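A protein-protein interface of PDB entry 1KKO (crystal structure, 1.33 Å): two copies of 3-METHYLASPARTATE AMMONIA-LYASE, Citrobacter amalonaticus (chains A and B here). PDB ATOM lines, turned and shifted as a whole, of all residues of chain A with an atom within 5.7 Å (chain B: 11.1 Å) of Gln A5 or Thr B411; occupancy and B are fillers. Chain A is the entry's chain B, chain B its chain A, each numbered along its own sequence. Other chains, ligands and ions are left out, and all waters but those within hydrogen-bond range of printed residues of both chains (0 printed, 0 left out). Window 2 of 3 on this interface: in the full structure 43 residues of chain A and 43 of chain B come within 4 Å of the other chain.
The side-chain amide nitrogen (NE2) of Gln A56 is in hydrogen-bond range of the backbone carbonyl oxygen (O) of Arg B404, 3.1 Å away.
The backbone carbonyl oxygen of Leu B408 sits at hydrogen-bond distance from the side-chain hydroxyl of Thr B411, 2.7 Å away.
The backbone NH of Lys A4 sits at hydrogen-bond distance from the backbone carbonyl oxygen of Ile A58 (2.7 Å).
The backbone carbonyl oxygen (O) of Gln A5 is in hydrogen-bond range of the backbone NH (N) of Ile A58, at 2.8 Å.
The backbone NH of Leu A7 is in hydrogen-bond range of the backbone carbonyl oxygen of Gln A56 (2.8 Å).
CB of Thr B411 touches OE1 of Gln A5, 3.7 Å away.
CD1 of Leu A7 touches O of Ala B407, 3.8 Å away.
Leu A7 touches Leu B408.
CD1 of Leu A7 touches CG2 of Thr B411, 3.6 Å away.
Gln A56 touches Leu B408 (OE1 to CD1, 3.2 Å).
Ile A58 touches Leu B408 (CD1 to CD2, 3.9 Å).
No residue of chain B comes within 4 Å of Lys A4.
Gln A5 touches one residue of chain B.
Leu A7 touches three residues of chain B.
Printed residues of chain B within 4 Å of Gln A56: Arg B404 and Leu B408.
Of the printed residues of chain B, Ile A58 touches Leu B408 (3.9 Å).
Asn B403 touches none of the printed residues of chain A.
Of the printed residues of chain A, Arg B404 touches Gln A56.
Of the printed residues of chain A, Leu B408 touches Leu A7 (3.98 Å), Gln A56 (3.2 Å) and Ile A58 (3.9 Å).
Gln B410 touches none of the printed residues of chain A.
Thr B411 touches two residues of chain A.
The nearest residue of chain B that does not touch Gln A5 is Ala B407 (6.6 Å).
The nearest residue of chain A that does not touch Thr B411 is Ile A58 (4.2 Å).
Of the 10 printed residues of chain A, 4 touch a printed residue of chain B.
Hydrophobic or aromatic side chains of chain A that line the printed part of chain B: Leu A7 and Ile A58.
Of the 17 printed residues of chain B, 4 touch a printed residue of chain A.
Among the printed residues, 7 pairs touch across the chains.
Among the printed residues, no Asp or Glu carboxylate lies within 4 Å of a Lys or Arg side-chain nitrogen of the other chain.
No position is printed for both chains.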
ATOM      1  N   ILE A   3      -9.724 -36.247  18.948  1.00  0.00           N
ATOM      2  CA  ILE A   3     -10.442 -35.177  18.280  1.00  0.00           C
ATOM      3  C   ILE A   3     -11.912 -35.581  18.202  1.00  0.00           C
ATOM      4  O   ILE A   3     -12.230 -36.693  17.762  1.00  0.00           O
ATOM      5  CB  ILE A   3      -9.906 -35.012  16.853  1.00  0.00           C
ATOM      6  CG1 ILE A   3      -8.451 -34.532  16.884  1.00  0.00           C
ATOM      7  CG2 ILE A   3     -10.796 -34.065  16.064  1.00  0.00           C
ATOM      8  CD1 ILE A   3      -7.745 -34.630  15.544  1.00  0.00           C
ATOM      9  N   LYS A   4     -12.801 -34.687  18.619  1.00  0.00           N
ATOM     10  CA  LYS A   4     -14.236 -34.926  18.512  1.00  0.00           C
ATOM     11  C   LYS A   4     -14.776 -34.420  17.177  1.00  0.00           C
ATOM     12  O   LYS A   4     -15.560 -35.093  16.511  1.00  0.00           O
ATOM     13  CB  LYS A   4     -14.964 -34.252  19.671  1.00  0.00           C
ATOM     14  N   GLN A   5     -14.353 -33.224  16.773  1.00  0.00           N
ATOM     15  CA  GLN A   5     -14.878 -32.621  15.560  1.00  0.00           C
ATOM     16  C   GLN A   5     -13.788 -31.811  14.869  1.00  0.00           C
ATOM     17  O   GLN A   5     -12.968 -31.174  15.534  1.00  0.00           O
ATOM     18  CB  GLN A   5     -16.079 -31.722  15.902  1.00  0.00           C
ATOM     19  CG  GLN A   5     -16.802 -31.092  14.707  1.00  0.00           C
ATOM     20  CD  GLN A   5     -18.177 -30.516  15.047  1.00  0.00           C
ATOM     21  OE1 GLN A   5     -18.531 -30.393  16.213  1.00  0.00           O
ATOM     22  NE2 GLN A   5     -18.945 -30.169  14.023  1.00  0.00           N
ATOM     23  N   ALA A   6     -13.788 -31.842  13.541  1.00  0.00           N
ATOM     24  CA  ALA A   6     -12.833 -31.073  12.753  1.00  0.00           C
ATOM     25  C   ALA A   6     -13.596 -30.102  11.886  1.00  0.00           C
ATOM     26  O   ALA A   6     -14.484 -30.504  11.129  1.00  0.00           O
ATOM     27  CB  ALA A   6     -11.992 -31.994  11.886  1.00  0.00           C
ATOM     28  N   LEU A   7     -13.244 -28.820  11.992  1.00  0.00           N
ATOM     29  CA  LEU A   7     -13.875 -27.781  11.202  1.00  0.00           C
ATOM     30  C   LEU A   7     -12.849 -27.119  10.293  1.00  0.00           C
ATOM     31  O   LEU A   7     -11.695 -26.942  10.677  1.00  0.00           O
ATOM     32  CB  LEU A   7     -14.470 -26.691  12.091  1.00  0.00           C
ATOM     33  CG  LEU A   7     -15.468 -27.103  13.168  1.00  0.00           C
ATOM     34  CD1 LEU A   7     -16.085 -25.870  13.810  1.00  0.00           C
ATOM     35  CD2 LEU A   7     -16.534 -28.003  12.608  1.00  0.00           C
ATOM     36  N   GLN A  56      -9.744 -26.259  12.695  1.00  0.00           N
ATOM     37  CA  GLN A  56     -10.036 -26.243  14.111  1.00  0.00           C
ATOM     38  C   GLN A  56     -10.405 -27.657  14.522  1.00  0.00           C
ATOM     39  O   GLN A  56     -11.298 -28.277  13.925  1.00  0.00           O
ATOM     40  CB  GLN A  56     -11.183 -25.294  14.407  1.00  0.00           C
ATOM     41  CG  GLN A  56     -10.838 -23.835  14.163  1.00  0.00           C
ATOM     42  CD  GLN A  56     -11.951 -22.905  14.578  1.00  0.00           C
ATOM     43  OE1 GLN A  56     -11.873 -22.260  15.627  1.00  0.00           O
ATOM     44  NE2 GLN A  56     -12.985 -22.833  13.763  1.00  0.00           N
ATOM     45  N   LEU A  57      -9.705 -28.150  15.534  1.00  0.00           N
ATOM     46  CA  LEU A  57      -9.929 -29.500  16.026  1.00  0.00           C
ATOM     47  C   LEU A  57     -10.449 -29.380  17.438  1.00  0.00           C
ATOM     48  O   LEU A  57      -9.720 -29.001  18.348  1.00  0.00           O
ATOM     49  CB  LEU A  57      -8.626 -30.296  16.016  1.00  0.00           C
ATOM     50  CG  LEU A  57      -7.866 -30.341  14.693  1.00  0.00           C
ATOM     51  CD1 LEU A  57      -6.556 -31.105  14.856  1.00  0.00           C
ATOM     52  CD2 LEU A  57      -8.707 -30.918  13.560  1.00  0.00           C
ATOM     53  N   ILE A  58     -11.730 -29.682  17.611  1.00  0.00           N
ATOM     54  CA  ILE A  58     -12.337 -29.661  18.933  1.00  0.00           C
ATOM     55  C   ILE A  58     -12.031 -31.010  19.568  1.00  0.00           C
ATOM     56  O   ILE A  58     -12.415 -32.051  19.028  1.00  0.00           O
ATOM     57  CB  ILE A  58     -13.858 -29.448  18.853  1.00  0.00           C
ATOM     58  CG1 ILE A  58     -14.209 -28.174  18.079  1.00  0.00           C
ATOM     59  CG2 ILE A  58     -14.457 -29.419  20.257  1.00  0.00           C
ATOM     60  CD1 ILE A  58     -15.712 -28.017  17.792  1.00  0.00           C
ATOM     61  N   LEU A  59     -11.342 -30.994  20.697  1.00  0.00           N
ATOM     62  CA  LEU A  59     -10.960 -32.223  21.381  1.00  0.00           C
ATOM     63  C   LEU A  59     -12.048 -32.654  22.352  1.00  0.00           C
ATOM     64  O   LEU A  59     -12.985 -31.899  22.636  1.00  0.00           O
ATOM     65  CB  LEU A  59      -9.668 -32.009  22.154  1.00  0.00           C
ATOM     66  CG  LEU A  59      -8.506 -31.423  21.341  1.00  0.00           C
ATOM     67  CD1 LEU A  59      -7.237 -31.466  22.166  1.00  0.00           C
ATOM     68  CD2 LEU A  59      -8.309 -32.150  20.012  1.00  0.00           C
ATOM     69  N   GLU A 102     -11.790 -37.069  12.694  1.00  0.00           N
ATOM     70  CA  GLU A 102     -12.790 -37.196  13.751  1.00  0.00           C
ATOM     71  C   GLU A 102     -12.650 -38.572  14.406  1.00  0.00           C
ATOM     72  O   GLU A 102     -12.758 -39.607  13.744  1.00  0.00           O
ATOM     73  CB  GLU A 102     -14.178 -36.851  13.208  1.00  0.00           C
ATOM     74  CG  GLU A 102     -14.197 -35.403  12.725  1.00  0.00           C
ATOM     75  CD  GLU A 102     -15.561 -34.863  12.356  1.00  0.00           C
ATOM     76  OE1 GLU A 102     -15.718 -33.618  12.387  1.00  0.00           O
ATOM     77  OE2 GLU A 102     -16.472 -35.660  12.024  1.00  0.00           O
ATOM     78  N   GLY B 147     -14.597 -24.019  29.560  1.00  0.00           N
ATOM     79  CA  GLY B 147     -14.927 -24.624  28.286  1.00  0.00           C
ATOM     80  C   GLY B 147     -15.807 -23.763  27.399  1.00  0.00           C
ATOM     81  O   GLY B 147     -16.563 -24.281  26.570  1.00  0.00           O
ATOM     82  N   ARG B 148     -15.718 -22.450  27.574  1.00  0.00           N
ATOM     83  CA  ARG B 148     -16.480 -21.533  26.748  1.00  0.00           C
ATOM     84  C   ARG B 148     -15.559 -20.704  25.884  1.00  0.00           C
ATOM     85  O   ARG B 148     -14.396 -20.554  26.197  1.00  0.00           O
ATOM     86  CB  ARG B 148     -17.288 -20.571  27.617  1.00  0.00           C
ATOM     87  CG  ARG B 148     -18.492 -21.202  28.298  1.00  0.00           C
ATOM     88  CD  ARG B 148     -19.264 -20.222  29.165  1.00  0.00           C
ATOM     89  NE  ARG B 148     -18.504 -19.850  30.345  1.00  0.00           N
ATOM     90  CZ  ARG B 148     -18.862 -18.917  31.222  1.00  0.00           C
ATOM     91  NH1 ARG B 148     -19.989 -18.244  31.041  1.00  0.00           N
ATOM     92  NH2 ARG B 148     -18.121 -18.663  32.280  1.00  0.00           N
ATOM     93  N   LEU B 149     -16.103 -20.174  24.802  1.00  0.00           N
ATOM     94  CA  LEU B 149     -15.375 -19.190  24.019  1.00  0.00           C
ATOM     95  C   LEU B 149     -15.523 -17.845  24.713  1.00  0.00           C
ATOM     96  O   LEU B 149     -16.483 -17.617  25.445  1.00  0.00           O
ATOM     97  CB  LEU B 149     -15.963 -19.078  22.625  1.00  0.00           C
ATOM     98  CG  LEU B 149     -16.131 -20.402  21.886  1.00  0.00           C
ATOM     99  CD1 LEU B 149     -16.607 -20.156  20.478  1.00  0.00           C
ATOM    100  CD2 LEU B 149     -14.843 -21.203  21.893  1.00  0.00           C
ATOM    101  N   THR B 151     -16.520 -15.136  23.474  1.00  0.00           N
ATOM    102  CA  THR B 151     -17.805 -14.575  23.071  1.00  0.00           C
ATOM    103  C   THR B 151     -18.920 -15.082  23.975  1.00  0.00           C
ATOM    104  O   THR B 151     -19.833 -14.332  24.335  1.00  0.00           O
ATOM    105  CB  THR B 151     -18.147 -14.952  21.617  1.00  0.00           C
ATOM    106  OG1 THR B 151     -18.193 -16.369  21.447  1.00  0.00           O
ATOM    107  CG2 THR B 151     -17.119 -14.553  20.694  1.00  0.00           C
ATOM    108  N   GLU B 152     -18.876 -16.370  24.296  1.00  0.00           N
ATOM    109  CA  GLU B 152     -19.922 -16.993  25.116  1.00  0.00           C
ATOM    110  C   GLU B 152     -19.912 -16.451  26.527  1.00  0.00           C
ATOM    111  O   GLU B 152     -20.968 -16.295  27.151  1.00  0.00           O
ATOM    112  CB  GLU B 152     -19.747 -18.511  25.127  1.00  0.00           C
ATOM    113  CG  GLU B 152     -20.039 -19.144  23.781  1.00  0.00           C
ATOM    114  CD  GLU B 152     -19.824 -20.637  23.790  1.00  0.00           C
ATOM    115  OE1 GLU B 152     -18.759 -21.080  24.246  1.00  0.00           O
ATOM    116  OE2 GLU B 152     -20.735 -21.373  23.364  1.00  0.00           O
ATOM    117  N   CYS B 162     -26.434 -14.151  21.660  1.00  0.00           N
ATOM    118  CA  CYS B 162     -25.315 -14.815  20.984  1.00  0.00           C
ATOM    119  C   CYS B 162     -25.649 -15.489  19.645  1.00  0.00           C
ATOM    120  O   CYS B 162     -25.167 -16.587  19.371  1.00  0.00           O
ATOM    121  CB  CYS B 162     -24.660 -15.849  21.914  1.00  0.00           C
ATOM    122  SG  CYS B 162     -22.960 -15.441  22.393  1.00  0.00           S
ATOM    123  N   VAL B 163     -26.456 -14.851  18.800  1.00  0.00           N
ATOM    124  CA  VAL B 163     -26.747 -15.402  17.475  1.00  0.00           C
ATOM    125  C   VAL B 163     -25.503 -15.228  16.593  1.00  0.00           C
ATOM    126  O   VAL B 163     -25.000 -14.112  16.477  1.00  0.00           O
ATOM    127  CB  VAL B 163     -27.965 -14.700  16.816  1.00  0.00           C
ATOM    128  CG1 VAL B 163     -28.222 -15.259  15.429  1.00  0.00           C
ATOM    129  CG2 VAL B 163     -29.206 -14.858  17.697  1.00  0.00           C
ATOM    130  N   PRO B 164     -24.999 -16.312  15.994  1.00  0.00           N
ATOM    131  CA  PRO B 164     -23.790 -16.243  15.162  1.00  0.00           C
ATOM    132  C   PRO B 164     -24.006 -15.466  13.879  1.00  0.00           C
ATOM    133  O   PRO B 164     -24.759 -15.898  13.006  1.00  0.00           O
ATOM    134  CB  PRO B 164     -23.481 -17.713  14.854  1.00  0.00           C
ATOM    135  CG  PRO B 164     -24.273 -18.490  15.805  1.00  0.00           C
ATOM    136  CD  PRO B 164     -25.508 -17.689  16.077  1.00  0.00           C
ATOM    137  N   ASN B 403     -14.717 -15.624  11.548  1.00  0.00           N
ATOM    138  CA  ASN B 403     -15.324 -16.779  10.890  1.00  0.00           C
ATOM    139  C   ASN B 403     -15.045 -18.109  11.579  1.00  0.00           C
ATOM    140  O   ASN B 403     -15.910 -18.983  11.605  1.00  0.00           O
ATOM    141  CB  ASN B 403     -14.990 -16.783   9.413  1.00  0.00           C
ATOM    142  CG  ASN B 403     -15.595 -15.591   8.698  1.00  0.00           C
ATOM    143  OD1 ASN B 403     -16.735 -15.223   8.965  1.00  0.00           O
ATOM    144  ND2 ASN B 403     -14.831 -14.971   7.803  1.00  0.00           N
ATOM    145  N   ARG B 404     -13.871 -18.252  12.175  1.00  0.00           N
ATOM    146  CA  ARG B 404     -13.584 -19.439  12.957  1.00  0.00           C
ATOM    147  C   ARG B 404     -14.553 -19.531  14.127  1.00  0.00           C
ATOM    148  O   ARG B 404     -15.058 -20.601  14.451  1.00  0.00           O
ATOM    149  CB  ARG B 404     -12.160 -19.411  13.526  1.00  0.00           C
ATOM    150  CG  ARG B 404     -11.062 -19.860  12.584  1.00  0.00           C
ATOM    151  CD  ARG B 404      -9.758 -20.082  13.307  1.00  0.00           C
ATOM    152  NE  ARG B 404      -9.194 -18.846  13.877  1.00  0.00           N
ATOM    153  CZ  ARG B 404      -8.397 -18.009  13.210  1.00  0.00           C
ATOM    154  NH1 ARG B 404      -8.083 -18.246  11.948  1.00  0.00           N
ATOM    155  NH2 ARG B 404      -7.909 -16.938  13.808  1.00  0.00           N
ATOM    156  N   THR B 405     -14.792 -18.398  14.762  1.00  0.00           N
ATOM    157  CA  THR B 405     -15.617 -18.357  15.956  1.00  0.00           C
ATOM    158  C   THR B 405     -17.082 -18.604  15.628  1.00  0.00           C
ATOM    159  O   THR B 405     -17.764 -19.335  16.353  1.00  0.00           O
ATOM    160  CB  THR B 405     -15.430 -17.027  16.671  1.00  0.00           C
ATOM    161  OG1 THR B 405     -14.053 -16.899  17.050  1.00  0.00           O
ATOM    162  CG2 THR B 405     -16.209 -16.994  17.990  1.00  0.00           C
ATOM    163  N   ILE B 406     -17.571 -18.016  14.546  1.00  0.00           N
ATOM    164  CA  ILE B 406     -18.931 -18.277  14.107  1.00  0.00           C
ATOM    165  C   ILE B 406     -19.082 -19.775  13.853  1.00  0.00           C
ATOM    166  O   ILE B 406     -20.085 -20.366  14.255  1.00  0.00           O
ATOM    167  CB  ILE B 406     -19.256 -17.451  12.871  1.00  0.00           C
ATOM    168  CG1 ILE B 406     -19.427 -15.988  13.281  1.00  0.00           C
ATOM    169  CG2 ILE B 406     -20.508 -17.978  12.172  1.00  0.00           C
ATOM    170  CD1 ILE B 406     -19.475 -15.010  12.152  1.00  0.00           C
ATOM    171  N   ALA B 407     -18.098 -20.401  13.208  1.00  0.00           N
ATOM    172  CA  ALA B 407     -18.181 -21.829  12.926  1.00  0.00           C
ATOM    173  C   ALA B 407     -18.244 -22.617  14.223  1.00  0.00           C
ATOM    174  O   ALA B 407     -19.022 -23.575  14.321  1.00  0.00           O
ATOM    175  CB  ALA B 407     -17.013 -22.286  12.098  1.00  0.00           C
ATOM    176  N   LEU B 408     -17.428 -22.264  15.213  1.00  0.00           N
ATOM    177  CA  LEU B 408     -17.473 -22.958  16.498  1.00  0.00           C
ATOM    178  C   LEU B 408     -18.847 -22.808  17.158  1.00  0.00           C
ATOM    179  O   LEU B 408     -19.423 -23.780  17.671  1.00  0.00           O
ATOM    180  CB  LEU B 408     -16.396 -22.447  17.456  1.00  0.00           C
ATOM    181  CG  LEU B 408     -14.954 -22.824  17.111  1.00  0.00           C
ATOM    182  CD1 LEU B 408     -14.024 -22.083  18.037  1.00  0.00           C
ATOM    183  CD2 LEU B 408     -14.753 -24.323  17.224  1.00  0.00           C
ATOM    184  N   LEU B 409     -19.370 -21.592  17.164  1.00  0.00           N
ATOM    185  CA  LEU B 409     -20.674 -21.333  17.780  1.00  0.00           C
ATOM    186  C   LEU B 409     -21.780 -22.156  17.122  1.00  0.00           C
ATOM    187  O   LEU B 409     -22.748 -22.546  17.777  1.00  0.00           O
ATOM    188  CB  LEU B 409     -21.019 -19.848  17.685  1.00  0.00           C
ATOM    189  CG  LEU B 409     -20.218 -18.930  18.606  1.00  0.00           C
ATOM    190  CD1 LEU B 409     -20.434 -17.495  18.197  1.00  0.00           C
ATOM    191  CD2 LEU B 409     -20.587 -19.133  20.063  1.00  0.00           C
ATOM    192  N   GLN B 410     -21.639 -22.414  15.831  1.00  0.00           N
ATOM    193  CA  GLN B 410     -22.646 -23.155  15.073  1.00  0.00           C
ATOM    194  C   GLN B 410     -22.633 -24.661  15.395  1.00  0.00           C
ATOM    195  O   GLN B 410     -23.599 -25.368  15.072  1.00  0.00           O
ATOM    196  CB  GLN B 410     -22.462 -22.897  13.570  1.00  0.00           C
ATOM    197  CG  GLN B 410     -22.958 -21.523  13.107  1.00  0.00           C
ATOM    198  CD  GLN B 410     -22.422 -21.105  11.733  1.00  0.00           C
ATOM    199  OE1 GLN B 410     -22.979 -20.211  11.083  1.00  0.00           O
ATOM    200  NE2 GLN B 410     -21.347 -21.738  11.297  1.00  0.00           N
ATOM    201  N   THR B 411     -21.573 -25.162  16.035  1.00  0.00           N
ATOM    202  CA  THR B 411     -21.524 -26.587  16.407  1.00  0.00           C
ATOM    203  C   THR B 411     -22.426 -26.850  17.608  1.00  0.00           C
ATOM    204  O   THR B 411     -22.912 -25.919  18.255  1.00  0.00           O
ATOM    205  CB  THR B 411     -20.093 -27.068  16.738  1.00  0.00           C
ATOM    206  OG1 THR B 411     -19.630 -26.455  17.949  1.00  0.00           O
ATOM    207  CG2 THR B 411     -19.107 -26.649  15.672  1.00  0.00           C
